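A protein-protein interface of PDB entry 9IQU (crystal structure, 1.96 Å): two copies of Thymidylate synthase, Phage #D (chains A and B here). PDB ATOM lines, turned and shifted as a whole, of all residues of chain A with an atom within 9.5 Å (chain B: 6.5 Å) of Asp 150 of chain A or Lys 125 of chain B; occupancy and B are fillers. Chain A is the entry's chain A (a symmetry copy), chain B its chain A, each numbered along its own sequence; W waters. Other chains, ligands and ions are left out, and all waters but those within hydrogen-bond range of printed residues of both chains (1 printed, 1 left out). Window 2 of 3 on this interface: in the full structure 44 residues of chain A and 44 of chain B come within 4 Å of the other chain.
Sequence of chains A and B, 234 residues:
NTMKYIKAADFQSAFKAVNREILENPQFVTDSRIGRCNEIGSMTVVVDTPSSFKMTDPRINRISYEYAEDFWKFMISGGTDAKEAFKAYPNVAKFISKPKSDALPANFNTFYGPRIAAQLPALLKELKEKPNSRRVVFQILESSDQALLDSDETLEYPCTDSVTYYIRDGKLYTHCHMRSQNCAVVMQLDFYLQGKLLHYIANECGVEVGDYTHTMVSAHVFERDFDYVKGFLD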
ATOM      1  N   ASP A 145     -30.667 -33.131  -5.057  1.00  0.00           N
ATOM      2  CA  ASP A 145     -31.293 -32.520  -6.200  1.00  0.00           C
ATOM      3  C   ASP A 145     -30.393 -31.492  -6.929  1.00  0.00           C
ATOM      4  O   ASP A 145     -30.711 -31.035  -8.010  1.00  0.00           O
ATOM      5  CB  ASP A 145     -32.596 -31.853  -5.772  1.00  0.00           C
ATOM      6  CG  ASP A 145     -33.598 -32.837  -5.172  1.00  0.00           C
ATOM      7  OD1 ASP A 145     -33.735 -33.947  -5.703  1.00  0.00           O
ATOM      8  OD2 ASP A 145     -34.231 -32.496  -4.168  1.00  0.00           O
ATOM      9  N   GLN A 146     -29.336 -31.093  -6.277  1.00  0.00           N
ATOM     10  CA  GLN A 146     -28.443 -30.116  -6.886  1.00  0.00           C
ATOM     11  C   GLN A 146     -27.755 -30.679  -8.151  1.00  0.00           C
ATOM     12  O   GLN A 146     -27.224 -29.947  -8.933  1.00  0.00           O
ATOM     13  CB  GLN A 146     -27.476 -29.581  -5.840  1.00  0.00           C
ATOM     14  CG  GLN A 146     -28.202 -28.726  -4.793  1.00  0.00           C
ATOM     15  CD  GLN A 146     -27.432 -28.484  -3.497  1.00  0.00           C
ATOM     16  OE1 GLN A 146     -26.222 -28.611  -3.443  1.00  0.00           O
ATOM     17  NE2 GLN A 146     -28.154 -28.102  -2.451  1.00  0.00           N
ATOM     18  N   ALA A 147     -27.828 -31.980  -8.316  1.00  0.00           N
ATOM     19  CA  ALA A 147     -27.261 -32.570  -9.534  1.00  0.00           C
ATOM     20  C   ALA A 147     -28.036 -32.117 -10.762  1.00  0.00           C
ATOM     21  O   ALA A 147     -27.515 -32.177 -11.853  1.00  0.00           O
ATOM     22  CB  ALA A 147     -27.138 -34.063  -9.423  1.00  0.00           C
ATOM     23  N   LEU A 148     -29.223 -31.570 -10.575  1.00  0.00           N
ATOM     24  CA  LEU A 148     -30.012 -31.039 -11.680  1.00  0.00           C
ATOM     25  C   LEU A 148     -29.585 -29.644 -12.154  1.00  0.00           C
ATOM     26  O   LEU A 148     -29.811 -29.282 -13.296  1.00  0.00           O
ATOM     27  CB  LEU A 148     -31.487 -30.972 -11.293  1.00  0.00           C
ATOM     28  CG  LEU A 148     -32.213 -32.291 -11.019  1.00  0.00           C
ATOM     29  CD1 LEU A 148     -33.578 -32.085 -10.374  1.00  0.00           C
ATOM     30  CD2 LEU A 148     -32.347 -33.077 -12.310  1.00  0.00           C
ATOM     31  N   LEU A 149     -28.911 -28.922 -11.288  1.00  0.00           N
ATOM     32  CA  LEU A 149     -28.579 -27.539 -11.608  1.00  0.00           C
ATOM     33  C   LEU A 149     -27.791 -27.348 -12.883  1.00  0.00           C
ATOM     34  O   LEU A 149     -28.127 -26.518 -13.670  1.00  0.00           O
ATOM     35  CB  LEU A 149     -27.821 -26.864 -10.481  1.00  0.00           C
ATOM     36  CG  LEU A 149     -28.626 -26.896  -9.175  1.00  0.00           C
ATOM     37  CD1 LEU A 149     -27.855 -26.396  -7.972  1.00  0.00           C
ATOM     38  CD2 LEU A 149     -29.933 -26.144  -9.334  1.00  0.00           C
ATOM     39  N   ASP A 150     -26.715 -28.069 -12.999  1.00  0.00           N
ATOM     40  CA  ASP A 150     -25.867 -27.937 -14.180  1.00  0.00           C
ATOM     41  C   ASP A 150     -26.208 -29.021 -15.183  1.00  0.00           C
ATOM     42  O   ASP A 150     -25.339 -29.509 -15.846  1.00  0.00           O
ATOM     43  CB  ASP A 150     -24.405 -28.009 -13.777  1.00  0.00           C
ATOM     44  CG  ASP A 150     -23.497 -27.395 -14.804  1.00  0.00           C
ATOM     45  OD1 ASP A 150     -23.947 -26.489 -15.528  1.00  0.00           O
ATOM     46  OD2 ASP A 150     -22.339 -27.816 -14.884  1.00  0.00           O
ATOM     47  N   SER A 151     -27.473 -29.373 -15.324  1.00  0.00           N
ATOM     48  CA  SER A 151     -27.890 -30.453 -16.213  1.00  0.00           C
ATOM     49  C   SER A 151     -28.816 -29.991 -17.308  1.00  0.00           C
ATOM     50  O   SER A 151     -29.230 -28.880 -17.354  1.00  0.00           O
ATOM     51  CB  SER A 151     -28.589 -31.575 -15.453  1.00  0.00           C
ATOM     52  OG  SER A 151     -29.974 -31.363 -15.336  1.00  0.00           O
ATOM     53  N   ASP A 152     -29.111 -30.860 -18.222  1.00  0.00           N
ATOM     54  CA  ASP A 152     -30.088 -30.496 -19.225  1.00  0.00           C
ATOM     55  C   ASP A 152     -31.299 -31.386 -19.056  1.00  0.00           C
ATOM     56  O   ASP A 152     -32.041 -31.635 -20.001  1.00  0.00           O
ATOM     57  CB  ASP A 152     -29.518 -30.538 -20.639  1.00  0.00           C
ATOM     58  CG  ASP A 152     -28.706 -31.800 -20.907  1.00  0.00           C
ATOM     59  OD1 ASP A 152     -28.661 -32.684 -20.036  1.00  0.00           O
ATOM     60  OD2 ASP A 152     -28.119 -31.915 -22.003  1.00  0.00           O
ATOM     61  N   GLU A 153     -31.514 -31.847 -17.845  1.00  0.00           N
ATOM     62  CA  GLU A 153     -32.733 -32.601 -17.603  1.00  0.00           C
ATOM     63  C   GLU A 153     -33.902 -31.608 -17.422  1.00  0.00           C
ATOM     64  O   GLU A 153     -33.674 -30.451 -17.158  1.00  0.00           O
ATOM     65  CB  GLU A 153     -32.546 -33.500 -16.404  1.00  0.00           C
ATOM     66  CG  GLU A 153     -31.484 -34.552 -16.618  1.00  0.00           C
ATOM     67  CD  GLU A 153     -32.044 -35.949 -16.617  1.00  0.00           C
ATOM     68  OE1 GLU A 153     -33.269 -36.111 -16.781  1.00  0.00           O
ATOM     69  OE2 GLU A 153     -31.253 -36.892 -16.452  1.00  0.00           O
ATOM     70  N   TYR A 157     -36.773 -29.288 -10.326  1.00  0.00           N
ATOM     71  CA  TYR A 157     -35.943 -29.061  -9.157  1.00  0.00           C
ATOM     72  C   TYR A 157     -36.913 -28.534  -8.087  1.00  0.00           C
ATOM     73  O   TYR A 157     -37.460 -27.447  -8.247  1.00  0.00           O
ATOM     74  CB  TYR A 157     -34.823 -28.069  -9.485  1.00  0.00           C
ATOM     75  CG  TYR A 157     -33.925 -27.656  -8.330  1.00  0.00           C
ATOM     76  CD1 TYR A 157     -32.849 -28.437  -7.947  1.00  0.00           C
ATOM     77  CD2 TYR A 157     -34.148 -26.472  -7.645  1.00  0.00           C
ATOM     78  CE1 TYR A 157     -32.028 -28.054  -6.916  1.00  0.00           C
ATOM     79  CE2 TYR A 157     -33.330 -26.073  -6.612  1.00  0.00           C
ATOM     80  CZ  TYR A 157     -32.267 -26.868  -6.247  1.00  0.00           C
ATOM     81  OH  TYR A 157     -31.438 -26.481  -5.213  1.00  0.00           O
ATOM     82  N   LEU B 120     -21.280 -25.977  -1.431  1.00  0.00           N
ATOM     83  CA  LEU B 120     -20.756 -24.684  -1.896  1.00  0.00           C
ATOM     84  C   LEU B 120     -20.417 -24.665  -3.386  1.00  0.00           C
ATOM     85  O   LEU B 120     -20.807 -23.724  -4.077  1.00  0.00           O
ATOM     86  CB  LEU B 120     -19.526 -24.264  -1.087  1.00  0.00           C
ATOM     87  CG  LEU B 120     -19.785 -23.188  -0.030  1.00  0.00           C
ATOM     88  CD1 LEU B 120     -18.589 -23.032   0.927  1.00  0.00           C
ATOM     89  CD2 LEU B 120     -20.140 -21.862  -0.687  1.00  0.00           C
ATOM     90  N   PRO B 121     -19.713 -25.697  -3.898  1.00  0.00           N
ATOM     91  CA  PRO B 121     -19.339 -25.576  -5.313  1.00  0.00           C
ATOM     92  C   PRO B 121     -20.531 -25.509  -6.280  1.00  0.00           C
ATOM     93  O   PRO B 121     -20.521 -24.675  -7.187  1.00  0.00           O
ATOM     94  CB  PRO B 121     -18.520 -26.845  -5.559  1.00  0.00           C
ATOM     95  CG  PRO B 121     -17.932 -27.167  -4.223  1.00  0.00           C
ATOM     96  CD  PRO B 121     -19.036 -26.846  -3.258  1.00  0.00           C
ATOM     97  N   ALA B 122     -21.539 -26.356  -6.081  1.00  0.00           N
ATOM     98  CA  ALA B 122     -22.675 -26.371  -6.991  1.00  0.00           C
ATOM     99  C   ALA B 122     -23.529 -25.118  -6.803  1.00  0.00           C
ATOM    100  O   ALA B 122     -23.978 -24.531  -7.769  1.00  0.00           O
ATOM    101  CB  ALA B 122     -23.533 -27.651  -6.791  1.00  0.00           C
ATOM    102  N   LEU B 123     -23.765 -24.722  -5.557  1.00  0.00           N
ATOM    103  CA  LEU B 123     -24.629 -23.575  -5.303  1.00  0.00           C
ATOM    104  C   LEU B 123     -23.959 -22.276  -5.777  1.00  0.00           C
ATOM    105  O   LEU B 123     -24.614 -21.448  -6.411  1.00  0.00           O
ATOM    106  CB  LEU B 123     -25.020 -23.509  -3.816  1.00  0.00           C
ATOM    107  CG  LEU B 123     -25.960 -24.670  -3.419  1.00  0.00           C
ATOM    108  CD1 LEU B 123     -26.453 -24.626  -1.985  1.00  0.00           C
ATOM    109  CD2 LEU B 123     -27.154 -24.823  -4.383  1.00  0.00           C
ATOM    110  N   LEU B 124     -22.660 -22.118  -5.526  1.00  0.00           N
ATOM    111  CA  LEU B 124     -21.936 -20.945  -6.020  1.00  0.00           C
ATOM    112  C   LEU B 124     -21.973 -20.885  -7.544  1.00  0.00           C
ATOM    113  O   LEU B 124     -22.124 -19.823  -8.117  1.00  0.00           O
ATOM    114  CB  LEU B 124     -20.487 -20.938  -5.527  1.00  0.00           C
ATOM    115  CG  LEU B 124     -20.234 -20.151  -4.237  1.00  0.00           C
ATOM    116  CD1 LEU B 124     -18.743 -20.091  -3.933  1.00  0.00           C
ATOM    117  CD2 LEU B 124     -20.815 -18.739  -4.359  1.00  0.00           C
ATOM    118  N   LYS B 125     -21.851 -22.036  -8.197  1.00  0.00           N
ATOM    119  CA  LYS B 125     -21.903 -22.075  -9.644  1.00  0.00           C
ATOM    120  C   LYS B 125     -23.247 -21.569 -10.158  1.00  0.00           C
ATOM    121  O   LYS B 125     -23.294 -20.708 -11.034  1.00  0.00           O
ATOM    122  CB  LYS B 125     -21.625 -23.485 -10.139  1.00  0.00           C
ATOM    123  CG  LYS B 125     -21.747 -23.629 -11.623  1.00  0.00           C
ATOM    124  CD  LYS B 125     -21.518 -25.065 -12.054  1.00  0.00           C
ATOM    125  CE  LYS B 125     -21.623 -25.160 -13.562  1.00  0.00           C
ATOM    126  NZ  LYS B 125     -20.739 -24.179 -14.253  1.00  0.00           N
ATOM    127  N   GLU B 126     -24.336 -22.088  -9.592  1.00  0.00           N
ATOM    128  CA  GLU B 126     -25.679 -21.651  -9.973  1.00  0.00           C
ATOM    129  C   GLU B 126     -25.844 -20.164  -9.689  1.00  0.00           C
ATOM    130  O   GLU B 126     -26.367 -19.405 -10.516  1.00  0.00           O
ATOM    131  CB  GLU B 126     -26.735 -22.475  -9.221  1.00  0.00           C
ATOM    132  CG  GLU B 126     -28.137 -21.973  -9.353  1.00  0.00           C
ATOM    133  CD  GLU B 126     -28.810 -22.419 -10.633  1.00  0.00           C
ATOM    134  OE1 GLU B 126     -28.223 -23.254 -11.357  1.00  0.00           O
ATOM    135  OE2 GLU B 126     -29.933 -21.937 -10.903  1.00  0.00           O
ATOM    136  N   LEU B 127     -25.365 -19.728  -8.524  1.00  0.00           N
ATOM    137  CA  LEU B 127     -25.551 -18.333  -8.127  1.00  0.00           C
ATOM    138  C   LEU B 127     -24.815 -17.357  -9.047  1.00  0.00           C
ATOM    139  O   LEU B 127     -25.349 -16.292  -9.390  1.00  0.00           O
ATOM    140  CB  LEU B 127     -25.099 -18.141  -6.678  1.00  0.00           C
ATOM    141  CG  LEU B 127     -25.506 -16.868  -5.945  1.00  0.00           C
ATOM    142  CD1 LEU B 127     -27.035 -16.734  -5.875  1.00  0.00           C
ATOM    143  CD2 LEU B 127     -24.920 -16.900  -4.546  1.00  0.00           C
ATOM    144  N   LYS B 128     -23.587 -17.702  -9.434  1.00  0.00           N
ATOM    145  CA  LYS B 128     -22.800 -16.840 -10.320  1.00  0.00           C
ATOM    146  C   LYS B 128     -23.175 -16.963 -11.804  1.00  0.00           C
ATOM    147  O   LYS B 128     -23.104 -15.988 -12.544  1.00  0.00           O
ATOM    148  CB  LYS B 128     -21.303 -17.140 -10.177  1.00  0.00           C
ATOM    149  CG  LYS B 128     -20.714 -16.803  -8.826  1.00  0.00           C
ATOM    150  CD  LYS B 128     -19.491 -17.647  -8.532  1.00  0.00           C
ATOM    151  CE  LYS B 128     -18.328 -16.801  -8.120  1.00  0.00           C
ATOM    152  NZ  LYS B 128     -17.150 -17.679  -7.780  1.00  0.00           N
ATOM    153  N   GLU B 129     -23.544 -18.163 -12.244  1.00  0.00           N
ATOM    154  CA  GLU B 129     -23.698 -18.429 -13.682  1.00  0.00           C
ATOM    155  C   GLU B 129     -25.131 -18.426 -14.216  1.00  0.00           C
ATOM    156  O   GLU B 129     -25.325 -18.163 -15.392  1.00  0.00           O
ATOM    157  CB  GLU B 129     -23.048 -19.768 -14.034  1.00  0.00           C
ATOM    158  CG  GLU B 129     -21.593 -19.853 -13.621  1.00  0.00           C
ATOM    159  CD  GLU B 129     -20.893 -21.064 -14.199  1.00  0.00           C
ATOM    160  OE1 GLU B 129     -21.580 -21.930 -14.788  1.00  0.00           O
ATOM    161  OE2 GLU B 129     -19.660 -21.165 -14.034  1.00  0.00           O
ATOM    162  N   LYS B 130     -26.130 -18.734 -13.388  1.00  0.00           N
ATOM    163  CA  LYS B 130     -27.509 -18.664 -13.878  1.00  0.00           C
ATOM    164  C   LYS B 130     -28.155 -17.366 -13.391  1.00  0.00           C
ATOM    165  O   LYS B 130     -28.427 -17.203 -12.196  1.00  0.00           O
ATOM    166  CB  LYS B 130     -28.326 -19.877 -13.445  1.00  0.00           C
ATOM    167  CG  LYS B 130     -27.689 -21.257 -13.744  1.00  0.00           C
ATOM    168  CD  LYS B 130     -27.568 -21.560 -15.228  1.00  0.00           C
ATOM    169  CE  LYS B 130     -27.363 -23.064 -15.505  1.00  0.00           C
ATOM    170  NZ  LYS B 130     -26.068 -23.618 -14.983  1.00  0.00           N
HETATM  171  O   HOH W   1     -30.159 -24.597 -12.909  1.00  0.00           O
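The side-chain amino group (NZ) of Lys 130 of chain B lies within salt-bridge range of the side-chain carboxylate (OD1) of Asp 150 of chain A (3.6 Å).
The side-chain amino group of Lys 125 of chain B lies within salt-bridge range of the side-chain carboxylate of Glu 129 of chain B.
Asp 145 of chain A touches none of the printed residues of chain B. Of the printed residues of chain B, Gln 146 of chain A touches Leu 123 (3.8 Å). Printed residues of chain B within 4 Å of Leu 149 of chain A: Leu 123 (3.98 Å), Glu 126 (3.7 Å) and Lys 130 (3.8 Å). Printed residues of chain B within 4 Å of Asp 150 of chain A: Lys 125 and Lys 130. Printed residues of chain A within 4 Å of Leu 123 of chain B: Gln 146 (3.8 Å) and Leu 149 (3.98 Å). Of chain A, only Asp 150 comes within 4 Å of Lys 125 of chain B. No residue of chain A comes within 4 Å of Glu 129 of chain B. Printed residues of chain A within 4 Å of Lys 130 of chain B: Leu 149 and Asp 150. The nearest residue of chain B that does not touch Asp 150 of chain A is Glu 129 of chain B (5.2 Å). The nearest residue of chain A that does not touch Lys 125 of chain B is Leu 149 of chain A (6.6 Å).
Of the 11 printed residues of chain B, 4 touch a printed residue of chain A. Along chain B the printed residues that touch a printed residue of chain A span positions 123 to 130. Printed residues of chain A that touch a printed residue of chain B: Gln 146, Leu 149 and Asp 150. Hydrophobic or aromatic side chains of chain A within 4 Å of the printed part of chain B: Leu 149. Among the printed residues, Asp or Glu carboxylates within 4 Å of a Lys or Arg side-chain nitrogen of the other chain: Asp 150 of chain A with Lys 130 of chain B (3.6 Å).
Among the printed residues, merely in contact across the chains: Gln 146 of chain A with Leu 123 of chain B (3.8 Å), Leu 149 of chain A with Leu 123 of chain B (3.98 Å), Leu 149 of chain A with Glu 126 of chain B (3.7 Å), Leu 149 of chain A with Lys 130 of chain B (3.8 Å) and Asp 150 of chain A with Lys 125 of chain B (3.1 Å).
No position is printed for both chains.
Water W1 lies within hydrogen-bond range of the side-chain carboxylate (OE1) of Glu 126 of chain B and the backbone carbonyl oxygen (O) of Leu 149 of chain A.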
